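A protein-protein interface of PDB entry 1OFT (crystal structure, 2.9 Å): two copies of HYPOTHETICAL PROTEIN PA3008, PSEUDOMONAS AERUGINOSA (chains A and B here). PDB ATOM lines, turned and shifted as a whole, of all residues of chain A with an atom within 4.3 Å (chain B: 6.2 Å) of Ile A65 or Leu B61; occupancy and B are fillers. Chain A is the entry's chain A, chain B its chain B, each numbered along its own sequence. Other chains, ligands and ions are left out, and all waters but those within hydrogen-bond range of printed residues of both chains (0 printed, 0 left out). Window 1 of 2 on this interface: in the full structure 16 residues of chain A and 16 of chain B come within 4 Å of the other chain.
The backbone carbonyl oxygen (O) of Leu B51 is in hydrogen-bond range of the side-chain sulfur (SG) of Cys B58, 3.6 Å away.
Ile A65 touches just these residues of chain B: Leu B61, Pro B64 and Ile B65. Leu B61 touches just these residues of chain A: Ile A65 (3.4 Å) and Leu A156 (3.4 Å). Of the printed residues of chain B, Leu A49 touches Leu B49 and Leu B51. Printed residues of chain A within 4 Å of Leu B49: Leu A49. Printed residues of chain B within 4 Å of Glu A68: Pro B64 (3.3 Å). Of the printed residues of chain A, Leu B51 touches Leu A49. His B57 touches none of the printed residues of chain A. The nearest residue of chain B that does not touch Ile A65 is Leu B62 (5.5 Å). The nearest printed residue of chain A that does not touch Ile B65 is Pro A64 (4.2 Å).
Leu B49 touches its own counterpart, Leu A49. Pro B64 touches its own counterpart, Pro A64. Ile A65 touches Pro B64, but with the chains exchanged Pro A64 does not touch Ile B65 (4.2 Å). Ile B65 touches its own counterpart, Ile A65. Positions printed for both chains: 49, 61, 62, 63, 64 and 65. Of the 9 pairs that touch across the chains among the printed residues, 5 have their exchanged pair printed and touching as well.
Hydrophobic or aromatic side chains of chain B that line the printed part of chain A: Leu B49, Leu B51, Leu B61, Pro B64 and Ile B65. Of the 11 printed residues of chain A, 6 touch a printed residue of chain B. Hydrophobic or aromatic side chains of chain A that line the printed part of chain B: Leu A49, Pro A64, Ile A65 and Leu A156. Among the printed residues, 9 pairs touch across the chains.
Among the printed residues, merely in contact across the chains: Ile A65 with Ile B65, Glu A68 with Pro B64, Leu A49 with Leu B49, Ile A65 with Leu B61, Leu A156 with Leu B61, Leu A61 with Ile B65, Pro A64 with Pro B64, Leu A49 with Leu B51 and Ile A65 with Pro B64.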
ATOM      1  N   LEU A  49     -20.178 -19.898  15.963  1.00  0.00           N
ATOM      2  CA  LEU A  49     -20.116 -20.555  17.260  1.00  0.00           C
ATOM      3  C   LEU A  49     -18.889 -20.000  17.965  1.00  0.00           C
ATOM      4  O   LEU A  49     -17.772 -20.074  17.435  1.00  0.00           O
ATOM      5  CB  LEU A  49     -19.953 -22.062  17.071  1.00  0.00           C
ATOM      6  CG  LEU A  49     -20.228 -23.041  18.213  1.00  0.00           C
ATOM      7  CD1 LEU A  49     -19.681 -24.386  17.798  1.00  0.00           C
ATOM      8  CD2 LEU A  49     -19.577 -22.616  19.497  1.00  0.00           C
ATOM      9  N   LEU A  61     -15.871 -29.238  24.053  1.00  0.00           N
ATOM     10  CA  LEU A  61     -17.211 -28.806  23.703  1.00  0.00           C
ATOM     11  C   LEU A  61     -17.393 -28.788  22.211  1.00  0.00           C
ATOM     12  O   LEU A  61     -18.520 -28.833  21.728  1.00  0.00           O
ATOM     13  CB  LEU A  61     -17.468 -27.403  24.237  1.00  0.00           C
ATOM     14  CG  LEU A  61     -18.365 -27.271  25.463  1.00  0.00           C
ATOM     15  CD1 LEU A  61     -18.200 -28.462  26.378  1.00  0.00           C
ATOM     16  CD2 LEU A  61     -18.020 -25.977  26.189  1.00  0.00           C
ATOM     17  N   LEU A  62     -16.294 -28.717  21.472  1.00  0.00           N
ATOM     18  CA  LEU A  62     -16.374 -28.673  20.019  1.00  0.00           C
ATOM     19  C   LEU A  62     -16.519 -30.068  19.392  1.00  0.00           C
ATOM     20  O   LEU A  62     -17.287 -30.252  18.438  1.00  0.00           O
ATOM     21  CB  LEU A  62     -15.134 -27.977  19.453  1.00  0.00           C
ATOM     22  CG  LEU A  62     -15.300 -27.078  18.226  1.00  0.00           C
ATOM     23  CD1 LEU A  62     -13.958 -26.984  17.546  1.00  0.00           C
ATOM     24  CD2 LEU A  62     -16.311 -27.645  17.253  1.00  0.00           C
ATOM     25  N   ALA A  63     -15.784 -31.040  19.928  1.00  0.00           N
ATOM     26  CA  ALA A  63     -15.826 -32.415  19.421  1.00  0.00           C
ATOM     27  C   ALA A  63     -17.228 -32.878  19.072  1.00  0.00           C
ATOM     28  O   ALA A  63     -17.529 -33.143  17.913  1.00  0.00           O
ATOM     29  CB  ALA A  63     -15.227 -33.363  20.419  1.00  0.00           C
ATOM     30  N   PRO A  64     -18.112 -32.981  20.065  1.00  0.00           N
ATOM     31  CA  PRO A  64     -19.453 -33.424  19.712  1.00  0.00           C
ATOM     32  C   PRO A  64     -20.039 -32.764  18.467  1.00  0.00           C
ATOM     33  O   PRO A  64     -20.639 -33.443  17.657  1.00  0.00           O
ATOM     34  CB  PRO A  64     -20.260 -33.125  20.979  1.00  0.00           C
ATOM     35  CG  PRO A  64     -19.509 -32.027  21.612  1.00  0.00           C
ATOM     36  CD  PRO A  64     -18.090 -32.476  21.440  1.00  0.00           C
ATOM     37  N   ILE A  65     -19.859 -31.457  18.295  1.00  0.00           N
ATOM     38  CA  ILE A  65     -20.437 -30.796  17.125  1.00  0.00           C
ATOM     39  C   ILE A  65     -19.778 -31.258  15.837  1.00  0.00           C
ATOM     40  O   ILE A  65     -20.468 -31.570  14.871  1.00  0.00           O
ATOM     41  CB  ILE A  65     -20.361 -29.255  17.215  1.00  0.00           C
ATOM     42  CG1 ILE A  65     -21.185 -28.755  18.409  1.00  0.00           C
ATOM     43  CG2 ILE A  65     -20.932 -28.645  15.975  1.00  0.00           C
ATOM     44  CD1 ILE A  65     -21.193 -27.238  18.588  1.00  0.00           C
ATOM     45  N   LEU A  66     -18.450 -31.311  15.806  1.00  0.00           N
ATOM     46  CA  LEU A  66     -17.771 -31.767  14.599  1.00  0.00           C
ATOM     47  C   LEU A  66     -18.149 -33.211  14.348  1.00  0.00           C
ATOM     48  O   LEU A  66     -18.442 -33.586  13.223  1.00  0.00           O
ATOM     49  CB  LEU A  66     -16.255 -31.652  14.734  1.00  0.00           C
ATOM     50  CG  LEU A  66     -15.710 -30.223  14.877  1.00  0.00           C
ATOM     51  CD1 LEU A  66     -14.210 -30.243  14.857  1.00  0.00           C
ATOM     52  CD2 LEU A  66     -16.207 -29.348  13.760  1.00  0.00           C
ATOM     53  N   ARG A  67     -18.170 -34.027  15.394  1.00  0.00           N
ATOM     54  CA  ARG A  67     -18.532 -35.435  15.239  1.00  0.00           C
ATOM     55  C   ARG A  67     -19.925 -35.618  14.622  1.00  0.00           C
ATOM     56  O   ARG A  67     -20.060 -36.311  13.633  1.00  0.00           O
ATOM     57  CB  ARG A  67     -18.434 -36.148  16.587  1.00  0.00           C
ATOM     58  CG  ARG A  67     -18.603 -37.653  16.508  1.00  0.00           C
ATOM     59  CD  ARG A  67     -18.025 -38.375  17.723  1.00  0.00           C
ATOM     60  NE  ARG A  67     -18.550 -37.883  18.990  1.00  0.00           N
ATOM     61  CZ  ARG A  67     -17.905 -37.027  19.783  1.00  0.00           C
ATOM     62  NH1 ARG A  67     -18.455 -36.629  20.928  1.00  0.00           N
ATOM     63  NH2 ARG A  67     -16.707 -36.571  19.438  1.00  0.00           N
ATOM     64  N   GLU A  68     -20.964 -35.009  15.181  1.00  0.00           N
ATOM     65  CA  GLU A  68     -22.292 -35.159  14.599  1.00  0.00           C
ATOM     66  C   GLU A  68     -22.203 -34.851  13.112  1.00  0.00           C
ATOM     67  O   GLU A  68     -22.663 -35.623  12.279  1.00  0.00           O
ATOM     68  CB  GLU A  68     -23.295 -34.197  15.242  1.00  0.00           C
ATOM     69  CG  GLU A  68     -24.408 -34.840  16.105  1.00  0.00           C
ATOM     70  CD  GLU A  68     -23.895 -35.335  17.457  1.00  0.00           C
ATOM     71  OE1 GLU A  68     -24.712 -35.654  18.352  1.00  0.00           O
ATOM     72  OE2 GLU A  68     -22.661 -35.412  17.628  1.00  0.00           O
ATOM     73  N   LEU A  69     -21.595 -33.723  12.779  1.00  0.00           N
ATOM     74  CA  LEU A  69     -21.467 -33.319  11.384  1.00  0.00           C
ATOM     75  C   LEU A  69     -20.692 -34.315  10.512  1.00  0.00           C
ATOM     76  O   LEU A  69     -21.026 -34.521   9.343  1.00  0.00           O
ATOM     77  CB  LEU A  69     -20.779 -31.956  11.293  1.00  0.00           C
ATOM     78  CG  LEU A  69     -21.445 -30.665  11.763  1.00  0.00           C
ATOM     79  CD1 LEU A  69     -20.363 -29.594  11.972  1.00  0.00           C
ATOM     80  CD2 LEU A  69     -22.469 -30.200  10.744  1.00  0.00           C
ATOM     81  N   LEU A 156     -20.203 -22.427   8.725  1.00  0.00           N
ATOM     82  CA  LEU A 156     -20.137 -22.338  10.175  1.00  0.00           C
ATOM     83  C   LEU A 156     -18.786 -21.767  10.530  1.00  0.00           C
ATOM     84  O   LEU A 156     -17.754 -22.324  10.158  1.00  0.00           O
ATOM     85  CB  LEU A 156     -20.270 -23.727  10.803  1.00  0.00           C
ATOM     86  CG  LEU A 156     -20.129 -23.820  12.322  1.00  0.00           C
ATOM     87  CD1 LEU A 156     -21.316 -23.139  12.970  1.00  0.00           C
ATOM     88  CD2 LEU A 156     -20.060 -25.277  12.766  1.00  0.00           C
ATOM     89  N   LEU B  49     -20.722 -20.443  25.649  1.00  0.00           N
ATOM     90  CA  LEU B  49     -20.919 -20.855  24.267  1.00  0.00           C
ATOM     91  C   LEU B  49     -21.924 -19.891  23.673  1.00  0.00           C
ATOM     92  O   LEU B  49     -23.024 -19.736  24.218  1.00  0.00           O
ATOM     93  CB  LEU B  49     -21.493 -22.267  24.236  1.00  0.00           C
ATOM     94  CG  LEU B  49     -21.521 -23.097  22.949  1.00  0.00           C
ATOM     95  CD1 LEU B  49     -22.484 -24.258  23.159  1.00  0.00           C
ATOM     96  CD2 LEU B  49     -21.983 -22.274  21.757  1.00  0.00           C
ATOM     97  N   LEU B  51     -24.055 -18.721  20.182  1.00  0.00           N
ATOM     98  CA  LEU B  51     -24.563 -19.181  18.892  1.00  0.00           C
ATOM     99  C   LEU B  51     -25.370 -18.110  18.175  1.00  0.00           C
ATOM    100  O   LEU B  51     -26.395 -17.644  18.684  1.00  0.00           O
ATOM    101  CB  LEU B  51     -25.441 -20.413  19.083  1.00  0.00           C
ATOM    102  CG  LEU B  51     -24.639 -21.652  19.484  1.00  0.00           C
ATOM    103  CD1 LEU B  51     -25.575 -22.714  20.048  1.00  0.00           C
ATOM    104  CD2 LEU B  51     -23.850 -22.171  18.274  1.00  0.00           C
ATOM    105  N   GLY B  56     -33.286 -21.514  14.407  1.00  0.00           N
ATOM    106  CA  GLY B  56     -33.411 -22.947  14.251  1.00  0.00           C
ATOM    107  C   GLY B  56     -32.063 -23.630  14.156  1.00  0.00           C
ATOM    108  O   GLY B  56     -31.801 -24.580  14.897  1.00  0.00           O
ATOM    109  N   HIS B  57     -31.201 -23.147  13.260  1.00  0.00           N
ATOM    110  CA  HIS B  57     -29.887 -23.754  13.088  1.00  0.00           C
ATOM    111  C   HIS B  57     -29.056 -23.690  14.365  1.00  0.00           C
ATOM    112  O   HIS B  57     -28.201 -24.549  14.605  1.00  0.00           O
ATOM    113  CB  HIS B  57     -29.119 -23.117  11.919  1.00  0.00           C
ATOM    114  CG  HIS B  57     -28.009 -23.982  11.406  1.00  0.00           C
ATOM    115  ND1 HIS B  57     -26.872 -24.251  12.142  1.00  0.00           N
ATOM    116  CD2 HIS B  57     -27.908 -24.728  10.280  1.00  0.00           C
ATOM    117  CE1 HIS B  57     -26.121 -25.125  11.492  1.00  0.00           C
ATOM    118  NE2 HIS B  57     -26.727 -25.432  10.360  1.00  0.00           N
ATOM    119  N   CYS B  58     -29.304 -22.683  15.191  1.00  0.00           N
ATOM    120  CA  CYS B  58     -28.574 -22.576  16.445  1.00  0.00           C
ATOM    121  C   CYS B  58     -28.938 -23.752  17.349  1.00  0.00           C
ATOM    122  O   CYS B  58     -28.074 -24.325  18.018  1.00  0.00           O
ATOM    123  CB  CYS B  58     -28.901 -21.264  17.161  1.00  0.00           C
ATOM    124  SG  CYS B  58     -28.180 -19.785  16.406  1.00  0.00           S
ATOM    125  N   LEU B  59     -30.218 -24.111  17.371  1.00  0.00           N
ATOM    126  CA  LEU B  59     -30.668 -25.226  18.199  1.00  0.00           C
ATOM    127  C   LEU B  59     -30.029 -26.509  17.704  1.00  0.00           C
ATOM    128  O   LEU B  59     -29.622 -27.371  18.486  1.00  0.00           O
ATOM    129  CB  LEU B  59     -32.194 -25.344  18.159  1.00  0.00           C
ATOM    130  CG  LEU B  59     -32.926 -24.342  19.066  1.00  0.00           C
ATOM    131  CD1 LEU B  59     -34.422 -24.390  18.798  1.00  0.00           C
ATOM    132  CD2 LEU B  59     -32.629 -24.654  20.535  1.00  0.00           C
ATOM    133  N   THR B  60     -29.936 -26.625  16.390  1.00  0.00           N
ATOM    134  CA  THR B  60     -29.330 -27.791  15.788  1.00  0.00           C
ATOM    135  C   THR B  60     -27.903 -27.942  16.276  1.00  0.00           C
ATOM    136  O   THR B  60     -27.503 -29.010  16.720  1.00  0.00           O
ATOM    137  CB  THR B  60     -29.324 -27.659  14.278  1.00  0.00           C
ATOM    138  OG1 THR B  60     -30.667 -27.767  13.803  1.00  0.00           O
ATOM    139  CG2 THR B  60     -28.455 -28.734  13.648  1.00  0.00           C
ATOM    140  N   LEU B  61     -27.139 -26.859  16.188  1.00  0.00           N
ATOM    141  CA  LEU B  61     -25.745 -26.859  16.612  1.00  0.00           C
ATOM    142  C   LEU B  61     -25.599 -27.156  18.080  1.00  0.00           C
ATOM    143  O   LEU B  61     -24.568 -27.639  18.516  1.00  0.00           O
ATOM    144  CB  LEU B  61     -25.116 -25.507  16.314  1.00  0.00           C
ATOM    145  CG  LEU B  61     -24.191 -25.463  15.108  1.00  0.00           C
ATOM    146  CD1 LEU B  61     -24.655 -26.405  14.013  1.00  0.00           C
ATOM    147  CD2 LEU B  61     -24.152 -24.042  14.615  1.00  0.00           C
ATOM    148  N   LEU B  62     -26.638 -26.863  18.842  1.00  0.00           N
ATOM    149  CA  LEU B  62     -26.611 -27.083  20.277  1.00  0.00           C
ATOM    150  C   LEU B  62     -26.845 -28.547  20.654  1.00  0.00           C
ATOM    151  O   LEU B  62     -26.124 -29.096  21.501  1.00  0.00           O
ATOM    152  CB  LEU B  62     -27.680 -26.217  20.949  1.00  0.00           C
ATOM    153  CG  LEU B  62     -27.362 -25.613  22.317  1.00  0.00           C
ATOM    154  CD1 LEU B  62     -28.660 -25.264  22.986  1.00  0.00           C
ATOM    155  CD2 LEU B  62     -26.616 -26.587  23.180  1.00  0.00           C
ATOM    156  N   ALA B  63     -27.856 -29.164  20.033  1.00  0.00           N
ATOM    157  CA  ALA B  63     -28.215 -30.561  20.311  1.00  0.00           C
ATOM    158  C   ALA B  63     -27.004 -31.469  20.553  1.00  0.00           C
ATOM    159  O   ALA B  63     -26.840 -31.999  21.646  1.00  0.00           O
ATOM    160  CB  ALA B  63     -29.075 -31.129  19.177  1.00  0.00           C
ATOM    161  N   PRO B  64     -26.122 -31.637  19.548  1.00  0.00           N
ATOM    162  CA  PRO B  64     -24.968 -32.509  19.773  1.00  0.00           C
ATOM    163  C   PRO B  64     -24.243 -32.263  21.073  1.00  0.00           C
ATOM    164  O   PRO B  64     -23.795 -33.219  21.702  1.00  0.00           O
ATOM    165  CB  PRO B  64     -24.088 -32.256  18.562  1.00  0.00           C
ATOM    166  CG  PRO B  64     -24.482 -30.883  18.135  1.00  0.00           C
ATOM    167  CD  PRO B  64     -25.963 -30.882  18.295  1.00  0.00           C
ATOM    168  N   ILE B  65     -24.134 -31.002  21.493  1.00  0.00           N
ATOM    169  CA  ILE B  65     -23.441 -30.712  22.750  1.00  0.00           C
ATOM    170  C   ILE B  65     -24.261 -31.193  23.936  1.00  0.00           C
ATOM    171  O   ILE B  65     -23.734 -31.897  24.807  1.00  0.00           O
ATOM    172  CB  ILE B  65     -23.112 -29.201  22.916  1.00  0.00           C
ATOM    173  CG1 ILE B  65     -22.152 -28.767  21.793  1.00  0.00           C
ATOM    174  CG2 ILE B  65     -22.430 -28.957  24.259  1.00  0.00           C
ATOM    175  CD1 ILE B  65     -21.774 -27.291  21.805  1.00  0.00           C
